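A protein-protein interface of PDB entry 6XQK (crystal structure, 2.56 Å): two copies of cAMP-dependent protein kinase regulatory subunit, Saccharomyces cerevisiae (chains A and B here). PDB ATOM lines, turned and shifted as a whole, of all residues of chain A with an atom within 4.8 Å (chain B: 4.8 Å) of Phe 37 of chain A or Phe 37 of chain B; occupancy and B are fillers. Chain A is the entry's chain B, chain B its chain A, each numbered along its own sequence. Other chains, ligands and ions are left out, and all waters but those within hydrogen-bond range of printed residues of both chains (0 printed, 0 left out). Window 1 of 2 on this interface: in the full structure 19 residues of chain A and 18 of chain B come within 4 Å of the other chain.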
ATOM      1  N   PHE A  17     -24.139  -1.113 -20.790  1.00  0.00           N
ATOM      2  CA  PHE A  17     -23.875   0.048 -21.626  1.00  0.00           C
ATOM      3  C   PHE A  17     -24.888   0.124 -22.763  1.00  0.00           C
ATOM      4  O   PHE A  17     -25.526   1.159 -22.921  1.00  0.00           O
ATOM      5  CB  PHE A  17     -22.435   0.021 -22.148  1.00  0.00           C
ATOM      6  CG  PHE A  17     -22.135   1.083 -23.176  1.00  0.00           C
ATOM      7  CD1 PHE A  17     -22.240   2.433 -22.859  1.00  0.00           C
ATOM      8  CD2 PHE A  17     -21.730   0.738 -24.453  1.00  0.00           C
ATOM      9  CE1 PHE A  17     -21.945   3.408 -23.800  1.00  0.00           C
ATOM     10  CE2 PHE A  17     -21.453   1.718 -25.396  1.00  0.00           C
ATOM     11  CZ  PHE A  17     -21.553   3.042 -25.064  1.00  0.00           C
ATOM     12  N   PHE A  29     -23.726  10.889 -28.713  1.00  0.00           N
ATOM     13  CA  PHE A  29     -23.336   9.534 -28.362  1.00  0.00           C
ATOM     14  C   PHE A  29     -21.964   9.472 -27.668  1.00  0.00           C
ATOM     15  O   PHE A  29     -21.849   8.833 -26.626  1.00  0.00           O
ATOM     16  CB  PHE A  29     -23.378   8.611 -29.608  1.00  0.00           C
ATOM     17  CG  PHE A  29     -23.031   7.157 -29.330  1.00  0.00           C
ATOM     18  CD1 PHE A  29     -21.712   6.727 -29.335  1.00  0.00           C
ATOM     19  CD2 PHE A  29     -24.022   6.235 -29.014  1.00  0.00           C
ATOM     20  CE1 PHE A  29     -21.393   5.410 -29.013  1.00  0.00           C
ATOM     21  CE2 PHE A  29     -23.700   4.908 -28.732  1.00  0.00           C
ATOM     22  CZ  PHE A  29     -22.388   4.507 -28.724  1.00  0.00           C
ATOM     23  N   LEU A  30     -20.931  10.114 -28.247  1.00  0.00           N
ATOM     24  CA  LEU A  30     -19.589  10.078 -27.688  1.00  0.00           C
ATOM     25  C   LEU A  30     -19.505  10.657 -26.292  1.00  0.00           C
ATOM     26  O   LEU A  30     -18.826  10.062 -25.434  1.00  0.00           O
ATOM     27  CB  LEU A  30     -18.564  10.769 -28.618  1.00  0.00           C
ATOM     28  CG  LEU A  30     -18.186  10.036 -29.872  1.00  0.00           C
ATOM     29  CD1 LEU A  30     -17.157  10.798 -30.616  1.00  0.00           C
ATOM     30  CD2 LEU A  30     -17.657   8.637 -29.567  1.00  0.00           C
ATOM     31  N   SER A  33     -21.339   8.367 -23.798  1.00  0.00           N
ATOM     32  CA  SER A  33     -20.568   7.151 -23.579  1.00  0.00           C
ATOM     33  C   SER A  33     -19.329   7.398 -22.733  1.00  0.00           C
ATOM     34  O   SER A  33     -19.047   6.613 -21.836  1.00  0.00           O
ATOM     35  CB  SER A  33     -20.200   6.506 -24.905  1.00  0.00           C
ATOM     36  OG  SER A  33     -21.365   6.277 -25.677  1.00  0.00           O
ATOM     37  N   ALA A  34     -18.599   8.497 -22.981  1.00  0.00           N
ATOM     38  CA  ALA A  34     -17.432   8.847 -22.167  1.00  0.00           C
ATOM     39  C   ALA A  34     -17.889   9.150 -20.734  1.00  0.00           C
ATOM     40  O   ALA A  34     -17.290   8.625 -19.796  1.00  0.00           O
ATOM     41  CB  ALA A  34     -16.713  10.045 -22.749  1.00  0.00           C
ATOM     42  N   ASN A  35     -18.991   9.906 -20.561  1.00  0.00           N
ATOM     43  CA  ASN A  35     -19.515  10.198 -19.226  1.00  0.00           C
ATOM     44  C   ASN A  35     -19.907   8.947 -18.491  1.00  0.00           C
ATOM     45  O   ASN A  35     -19.589   8.818 -17.318  1.00  0.00           O
ATOM     46  CB  ASN A  35     -20.681  11.157 -19.276  1.00  0.00           C
ATOM     47  CG  ASN A  35     -20.291  12.573 -19.625  1.00  0.00           C
ATOM     48  OD1 ASN A  35     -19.112  12.916 -19.782  1.00  0.00           O
ATOM     49  ND2 ASN A  35     -21.290  13.432 -19.776  1.00  0.00           N
ATOM     50  N   TYR A  36     -20.553   8.003 -19.187  1.00  0.00           N
ATOM     51  CA  TYR A  36     -20.987   6.718 -18.629  1.00  0.00           C
ATOM     52  C   TYR A  36     -19.796   5.892 -18.099  1.00  0.00           C
ATOM     53  O   TYR A  36     -19.829   5.429 -16.956  1.00  0.00           O
ATOM     54  CB  TYR A  36     -21.797   5.918 -19.676  1.00  0.00           C
ATOM     55  CG  TYR A  36     -22.166   4.531 -19.198  1.00  0.00           C
ATOM     56  CD1 TYR A  36     -23.288   4.323 -18.415  1.00  0.00           C
ATOM     57  CD2 TYR A  36     -21.358   3.429 -19.486  1.00  0.00           C
ATOM     58  CE1 TYR A  36     -23.603   3.058 -17.930  1.00  0.00           C
ATOM     59  CE2 TYR A  36     -21.659   2.164 -19.000  1.00  0.00           C
ATOM     60  CZ  TYR A  36     -22.784   1.980 -18.227  1.00  0.00           C
ATOM     61  OH  TYR A  36     -23.071   0.716 -17.761  1.00  0.00           O
ATOM     62  N   PHE A  37     -18.767   5.702 -18.919  1.00  0.00           N
ATOM     63  CA  PHE A  37     -17.621   4.892 -18.540  1.00  0.00           C
ATOM     64  C   PHE A  37     -16.767   5.559 -17.474  1.00  0.00           C
ATOM     65  O   PHE A  37     -16.254   4.865 -16.584  1.00  0.00           O
ATOM     66  CB  PHE A  37     -16.808   4.462 -19.766  1.00  0.00           C
ATOM     67  CG  PHE A  37     -17.506   3.348 -20.493  1.00  0.00           C
ATOM     68  CD1 PHE A  37     -17.744   2.137 -19.867  1.00  0.00           C
ATOM     69  CD2 PHE A  37     -18.003   3.533 -21.778  1.00  0.00           C
ATOM     70  CE1 PHE A  37     -18.401   1.104 -20.532  1.00  0.00           C
ATOM     71  CE2 PHE A  37     -18.659   2.503 -22.440  1.00  0.00           C
ATOM     72  CZ  PHE A  37     -18.856   1.291 -21.810  1.00  0.00           C
ATOM     73  N   ASN A  38     -16.656   6.882 -17.513  1.00  0.00           N
ATOM     74  CA  ASN A  38     -15.917   7.612 -16.492  1.00  0.00           C
ATOM     75  C   ASN A  38     -16.629   7.506 -15.162  1.00  0.00           C
ATOM     76  O   ASN A  38     -15.971   7.459 -14.128  1.00  0.00           O
ATOM     77  CB  ASN A  38     -15.753   9.069 -16.882  1.00  0.00           C
ATOM     78  CG  ASN A  38     -14.739   9.306 -17.958  1.00  0.00           C
ATOM     79  OD1 ASN A  38     -13.718   8.640 -18.052  1.00  0.00           O
ATOM     80  ND2 ASN A  38     -14.995  10.279 -18.781  1.00  0.00           N
ATOM     81  N   LYS A  39     -17.978   7.471 -15.170  1.00  0.00           N
ATOM     82  CA  LYS A  39     -18.769   7.328 -13.966  1.00  0.00           C
ATOM     83  C   LYS A  39     -18.700   5.883 -13.459  1.00  0.00           C
ATOM     84  O   LYS A  39     -18.600   5.697 -12.255  1.00  0.00           O
ATOM     85  CB  LYS A  39     -20.221   7.757 -14.193  1.00  0.00           C
ATOM     86  CG  LYS A  39     -20.994   7.856 -12.880  1.00  0.00           C
ATOM     87  CD  LYS A  39     -22.380   8.362 -13.102  1.00  0.00           C
ATOM     88  CE  LYS A  39     -23.225   8.225 -11.867  1.00  0.00           C
ATOM     89  NZ  LYS A  39     -24.688   8.122 -12.182  1.00  0.00           N
ATOM     90  N   ARG A  40     -18.687   4.859 -14.355  1.00  0.00           N
ATOM     91  CA  ARG A  40     -18.550   3.460 -13.928  1.00  0.00           C
ATOM     92  C   ARG A  40     -17.206   3.258 -13.219  1.00  0.00           C
ATOM     93  O   ARG A  40     -17.137   2.506 -12.248  1.00  0.00           O
ATOM     94  CB  ARG A  40     -18.654   2.489 -15.118  1.00  0.00           C
ATOM     95  CG  ARG A  40     -20.067   2.299 -15.676  1.00  0.00           C
ATOM     96  CD  ARG A  40     -21.006   1.588 -14.712  1.00  0.00           C
ATOM     97  NE  ARG A  40     -20.559   0.233 -14.377  1.00  0.00           N
ATOM     98  CZ  ARG A  40     -20.189  -0.140 -13.162  1.00  0.00           C
ATOM     99  NH1 ARG A  40     -20.217   0.729 -12.153  1.00  0.00           N
ATOM    100  NH2 ARG A  40     -19.806  -1.385 -12.936  1.00  0.00           N
ATOM    101  N   LEU A  41     -16.142   3.911 -13.705  1.00  0.00           N
ATOM    102  CA  LEU A  41     -14.830   3.860 -13.084  1.00  0.00           C
ATOM    103  C   LEU A  41     -14.876   4.547 -11.722  1.00  0.00           C
ATOM    104  O   LEU A  41     -14.303   4.046 -10.764  1.00  0.00           O
ATOM    105  CB  LEU A  41     -13.791   4.568 -13.961  1.00  0.00           C
ATOM    106  CG  LEU A  41     -13.292   3.802 -15.194  1.00  0.00           C
ATOM    107  CD1 LEU A  41     -12.312   4.631 -15.950  1.00  0.00           C
ATOM    108  CD2 LEU A  41     -12.650   2.461 -14.802  1.00  0.00           C
ATOM    109  N   PHE B  17     -17.034   0.594 -31.552  1.00  0.00           N
ATOM    110  CA  PHE B  17     -16.685   0.257 -30.173  1.00  0.00           C
ATOM    111  C   PHE B  17     -16.739  -1.252 -29.956  1.00  0.00           C
ATOM    112  O   PHE B  17     -15.774  -1.824 -29.470  1.00  0.00           O
ATOM    113  CB  PHE B  17     -17.596   0.989 -29.196  1.00  0.00           C
ATOM    114  CG  PHE B  17     -17.450   0.543 -27.767  1.00  0.00           C
ATOM    115  CD1 PHE B  17     -16.256   0.710 -27.092  1.00  0.00           C
ATOM    116  CD2 PHE B  17     -18.530   0.020 -27.076  1.00  0.00           C
ATOM    117  CE1 PHE B  17     -16.133   0.337 -25.759  1.00  0.00           C
ATOM    118  CE2 PHE B  17     -18.408  -0.354 -25.750  1.00  0.00           C
ATOM    119  CZ  PHE B  17     -17.203  -0.204 -25.103  1.00  0.00           C
ATOM    120  N   PHE B  29     -12.289  -4.086 -18.872  1.00  0.00           N
ATOM    121  CA  PHE B  29     -13.304  -3.571 -19.791  1.00  0.00           C
ATOM    122  C   PHE B  29     -13.626  -2.101 -19.550  1.00  0.00           C
ATOM    123  O   PHE B  29     -13.621  -1.343 -20.504  1.00  0.00           O
ATOM    124  CB  PHE B  29     -14.590  -4.443 -19.731  1.00  0.00           C
ATOM    125  CG  PHE B  29     -15.670  -4.028 -20.708  1.00  0.00           C
ATOM    126  CD1 PHE B  29     -16.593  -3.050 -20.374  1.00  0.00           C
ATOM    127  CD2 PHE B  29     -15.748  -4.599 -21.964  1.00  0.00           C
ATOM    128  CE1 PHE B  29     -17.556  -2.634 -21.284  1.00  0.00           C
ATOM    129  CE2 PHE B  29     -16.729  -4.196 -22.865  1.00  0.00           C
ATOM    130  CZ  PHE B  29     -17.626  -3.213 -22.522  1.00  0.00           C
ATOM    131  N   LEU B  30     -13.915  -1.698 -18.300  1.00  0.00           N
ATOM    132  CA  LEU B  30     -14.262  -0.313 -18.000  1.00  0.00           C
ATOM    133  C   LEU B  30     -13.149   0.668 -18.316  1.00  0.00           C
ATOM    134  O   LEU B  30     -13.433   1.724 -18.874  1.00  0.00           O
ATOM    135  CB  LEU B  30     -14.743  -0.118 -16.564  1.00  0.00           C
ATOM    136  CG  LEU B  30     -16.085  -0.725 -16.181  1.00  0.00           C
ATOM    137  CD1 LEU B  30     -16.382  -0.451 -14.708  1.00  0.00           C
ATOM    138  CD2 LEU B  30     -17.207  -0.210 -17.088  1.00  0.00           C
ATOM    139  N   SER B  33     -12.770   0.911 -22.152  1.00  0.00           N
ATOM    140  CA  SER B  33     -13.913   1.607 -22.720  1.00  0.00           C
ATOM    141  C   SER B  33     -13.880   3.102 -22.428  1.00  0.00           C
ATOM    142  O   SER B  33     -14.142   3.884 -23.325  1.00  0.00           O
ATOM    143  CB  SER B  33     -15.214   0.997 -22.223  1.00  0.00           C
ATOM    144  OG  SER B  33     -15.219  -0.388 -22.510  1.00  0.00           O
ATOM    145  N   ALA B  34     -13.516   3.505 -21.211  1.00  0.00           N
ATOM    146  CA  ALA B  34     -13.387   4.919 -20.872  1.00  0.00           C
ATOM    147  C   ALA B  34     -12.258   5.540 -21.720  1.00  0.00           C
ATOM    148  O   ALA B  34     -12.468   6.586 -22.323  1.00  0.00           O
ATOM    149  CB  ALA B  34     -13.091   5.095 -19.387  1.00  0.00           C
ATOM    150  N   ASN B  35     -11.102   4.854 -21.828  1.00  0.00           N
ATOM    151  CA  ASN B  35     -10.003   5.354 -22.641  1.00  0.00           C
ATOM    152  C   ASN B  35     -10.398   5.508 -24.110  1.00  0.00           C
ATOM    153  O   ASN B  35     -10.017   6.495 -24.748  1.00  0.00           O
ATOM    154  CB  ASN B  35      -8.780   4.458 -22.516  1.00  0.00           C
ATOM    155  CG  ASN B  35      -8.091   4.519 -21.174  1.00  0.00           C
ATOM    156  OD1 ASN B  35      -8.465   5.277 -20.271  1.00  0.00           O
ATOM    157  ND2 ASN B  35      -7.079   3.704 -21.001  1.00  0.00           N
ATOM    158  N   TYR B  36     -11.172   4.541 -24.633  1.00  0.00           N
ATOM    159  CA  TYR B  36     -11.638   4.564 -26.017  1.00  0.00           C
ATOM    160  C   TYR B  36     -12.549   5.799 -26.316  1.00  0.00           C
ATOM    161  O   TYR B  36     -12.334   6.527 -27.302  1.00  0.00           O
ATOM    162  CB  TYR B  36     -12.370   3.241 -26.354  1.00  0.00           C
ATOM    163  CG  TYR B  36     -12.991   3.246 -27.742  1.00  0.00           C
ATOM    164  CD1 TYR B  36     -12.241   2.914 -28.865  1.00  0.00           C
ATOM    165  CD2 TYR B  36     -14.305   3.654 -27.938  1.00  0.00           C
ATOM    166  CE1 TYR B  36     -12.772   3.013 -30.148  1.00  0.00           C
ATOM    167  CE2 TYR B  36     -14.861   3.718 -29.214  1.00  0.00           C
ATOM    168  CZ  TYR B  36     -14.093   3.390 -30.317  1.00  0.00           C
ATOM    169  OH  TYR B  36     -14.640   3.473 -31.574  1.00  0.00           O
ATOM    170  N   PHE B  37     -13.566   6.010 -25.477  1.00  0.00           N
ATOM    171  CA  PHE B  37     -14.515   7.102 -25.660  1.00  0.00           C
ATOM    172  C   PHE B  37     -13.912   8.467 -25.404  1.00  0.00           C
ATOM    173  O   PHE B  37     -14.226   9.426 -26.128  1.00  0.00           O
ATOM    174  CB  PHE B  37     -15.782   6.860 -24.846  1.00  0.00           C
ATOM    175  CG  PHE B  37     -16.639   5.826 -25.543  1.00  0.00           C
ATOM    176  CD1 PHE B  37     -17.156   6.065 -26.813  1.00  0.00           C
ATOM    177  CD2 PHE B  37     -16.876   4.601 -24.965  1.00  0.00           C
ATOM    178  CE1 PHE B  37     -17.931   5.113 -27.460  1.00  0.00           C
ATOM    179  CE2 PHE B  37     -17.650   3.646 -25.623  1.00  0.00           C
ATOM    180  CZ  PHE B  37     -18.159   3.906 -26.869  1.00  0.00           C
ATOM    181  N   ASN B  38     -12.984   8.550 -24.445  1.00  0.00           N
ATOM    182  CA  ASN B  38     -12.264   9.782 -24.186  1.00  0.00           C
ATOM    183  C   ASN B  38     -11.358  10.119 -25.379  1.00  0.00           C
ATOM    184  O   ASN B  38     -11.179  11.306 -25.678  1.00  0.00           O
ATOM    185  CB  ASN B  38     -11.456   9.674 -22.918  1.00  0.00           C
ATOM    186  CG  ASN B  38     -12.289   9.744 -21.660  1.00  0.00           C
ATOM    187  OD1 ASN B  38     -13.299  10.446 -21.578  1.00  0.00           O
ATOM    188  ND2 ASN B  38     -11.886   9.025 -20.636  1.00  0.00           N
ATOM    189  N   LYS B  39     -10.805   9.092 -26.078  1.00  0.00           N
ATOM    190  CA  LYS B  39      -9.976   9.302 -27.262  1.00  0.00           C
ATOM    191  C   LYS B  39     -10.847   9.674 -28.466  1.00  0.00           C
ATOM    192  O   LYS B  39     -10.434  10.522 -29.248  1.00  0.00           O
ATOM    193  CB  LYS B  39      -9.122   8.083 -27.585  1.00  0.00           C
ATOM    194  CG  LYS B  39      -8.088   8.375 -28.663  1.00  0.00           C
ATOM    195  CD  LYS B  39      -7.253   7.137 -29.012  1.00  0.00           C
ATOM    196  CE  LYS B  39      -6.289   7.439 -30.117  1.00  0.00           C
ATOM    197  NZ  LYS B  39      -5.475   8.606 -29.741  1.00  0.00           N
ATOM    198  N   ARG B  40     -12.055   9.095 -28.610  1.00  0.00           N
ATOM    199  CA  ARG B  40     -12.954   9.472 -29.709  1.00  0.00           C
ATOM    200  C   ARG B  40     -13.360  10.948 -29.586  1.00  0.00           C
ATOM    201  O   ARG B  40     -13.458  11.655 -30.589  1.00  0.00           O
ATOM    202  CB  ARG B  40     -14.207   8.577 -29.724  1.00  0.00           C
ATOM    203  CG  ARG B  40     -13.974   7.153 -30.242  1.00  0.00           C
ATOM    204  CD  ARG B  40     -13.613   7.112 -31.726  1.00  0.00           C
ATOM    205  NE  ARG B  40     -14.674   7.658 -32.584  1.00  0.00           N
ATOM    206  CZ  ARG B  40     -14.573   8.779 -33.314  1.00  0.00           C
ATOM    207  NH1 ARG B  40     -13.446   9.483 -33.316  1.00  0.00           N
ATOM    208  NH2 ARG B  40     -15.598   9.200 -34.045  1.00  0.00           N
ATOM    209  N   LEU B  41     -13.580  11.410 -28.361  1.00  0.00           N
ATOM    210  CA  LEU B  41     -13.884  12.809 -28.090  1.00  0.00           C
ATOM    211  C   LEU B  41     -12.671  13.670 -28.435  1.00  0.00           C
ATOM    212  O   LEU B  41     -12.828  14.742 -29.027  1.00  0.00           O
ATOM    213  CB  LEU B  41     -14.219  13.006 -26.594  1.00  0.00           C
ATOM    214  CG  LEU B  41     -15.599  12.578 -26.119  1.00  0.00           C
ATOM    215  CD1 LEU B  41     -15.742  12.840 -24.637  1.00  0.00           C
ATOM    216  CD2 LEU B  41     -16.683  13.320 -26.874  1.00  0.00           C
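OG of Ser 33 of chain B sits at hydrogen-bond distance from O of Phe 29 of chain B (2.7 Å). The side-chain amide nitrogen of Asn 38 of chain B lies within hydrogen-bond range of the backbone carbonyl oxygen of Ala 34 of chain B (3.0 Å). OG of Ser 33 of chain A lies within hydrogen-bond range of O of Phe 29 of chain A, at 2.8 Å. O of Ala 34 of chain A lies within hydrogen-bond range of ND2 of Asn 38 of chain A, at 3.0 Å.
Among the printed residues, merely in contact across the chains: Leu 30 of chain A with Arg 40 of chain B (3.5 Å), Ala 34 of chain A with Leu 41 of chain B (3.5 Å), Phe 37 of chain A with Phe 37 of chain B (3.5 Å), Leu 41 of chain A with Ala 34 of chain B (3.6 Å), Phe 37 of chain A with Ser 33 of chain B (3.6 Å), Leu 30 of chain A with Leu 41 of chain B (3.6 Å), Ser 33 of chain A with Phe 37 of chain B (3.6 Å), Phe 37 of chain A with Ala 34 of chain B (3.6 Å), Ala 34 of chain A with Asn 38 of chain B (3.6 Å), Arg 40 of chain A with Leu 30 of chain B (3.6 Å), Phe 37 of chain A with Leu 30 of chain B (3.7 Å), Phe 17 of chain A with Phe 17 of chain B (3.7 Å), Ala 34 of chain A with Phe 37 of chain B (3.7 Å), Leu 41 of chain A with Leu 30 of chain B (3.8 Å), Leu 30 of chain A with Phe 37 of chain B (3.8 Å), Phe 29 of chain A with Phe 37 of chain B (3.8 Å), Asn 38 of chain A with Ala 34 of chain B (3.8 Å), Phe 37 of chain A with Phe 29 of chain B (3.9 Å), Phe 17 of chain A with Phe 37 of chain B (3.9 Å) and Phe 37 of chain A with Phe 17 of chain B (3.98 Å).
Of the 12 printed residues of chain B, 9 touch a printed residue of chain A. Printed residues of chain B that touch a printed residue of chain A: Phe 17, Phe 29, Leu 30, Ser 33, Ala 34, Phe 37, Asn 38, Arg 40 and Leu 41. Of the 12 printed residues of chain A, 9 touch a printed residue of chain B. Printed residues of chain A that touch a printed residue of chain B: Phe 17, Phe 29, Leu 30, Ser 33, Ala 34, Phe 37, Asn 38, Arg 40 and Leu 41. Hydrophobic or aromatic side chains of chain A within 4 Å of the printed part of chain B: Phe 17, Phe 29, Leu 30, Ala 34, Phe 37 and Leu 41. Along chain A the printed residues that touch a printed residue of chain B span positions 17 to 41. Among the printed residues, 21 pairs touch across the chains. Among the printed residues, no Asp or Glu carboxylate lies within 4 Å of a Lys or Arg side-chain nitrogen of the other chain.
Phe 29 of chain A touches Phe 37 of chain B, and with the chains exchanged Phe 37 of chain A touches Phe 29 of chain B. Ser 33 of chain A touches Phe 37 of chain B, and with the chains exchanged Phe 37 of chain A touches Ser 33 of chain B. Ala 34 of chain A touches Phe 37 of chain B, and with the chains exchanged Phe 37 of chain A touches Ala 34 of chain B. Ala 34 of chain A touches Asn 38 of chain B, and with the chains exchanged Asn 38 of chain A touches Ala 34 of chain B. Positions printed for both chains: 17, 29, 30, 33, 34, 35, 36, 37, 38, 39, 40 and 41. Of the 21 pairs that touch across the chains among the printed residues, 21 have their exchanged pair printed and touching as well.
Phe 37 of chain A touches just these residues of chain B: Phe 17 (3.98 Å), Phe 29 (3.9 Å), Leu 30 (3.7 Å), Ser 33 (3.6 Å), Ala 34 (3.6 Å) and Phe 37 (3.5 Å). Phe 37 of chain B touches six residues of chain A. Of the printed residues of chain B, Leu 41 of chain A touches Leu 30 (3.8 Å) and Ala 34 (3.6 Å). Of the printed residues of chain A, Ala 34 of chain B touches Phe 37 (3.6 Å), Asn 38 (3.8 Å) and Leu 41 (3.6 Å). Of the printed residues of chain A, Leu 41 of chain B touches Leu 30 and Ala 34. Of the printed residues of chain A, Asn 38 of chain B touches Ala 34 and Asn 38. The nearest printed residue of chain A that does not touch Phe 37 of chain B is Asn 35 of chain A (6.2 Å). The nearest printed residue of chain A that does not touch Leu 41 of chain B is Asn 35 of chain A (5.9 Å).
ND2 of Asn 38 of chain B is in hydrogen-bond range of OD1 of Asn 38 of chain A, 3.2 Å away.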
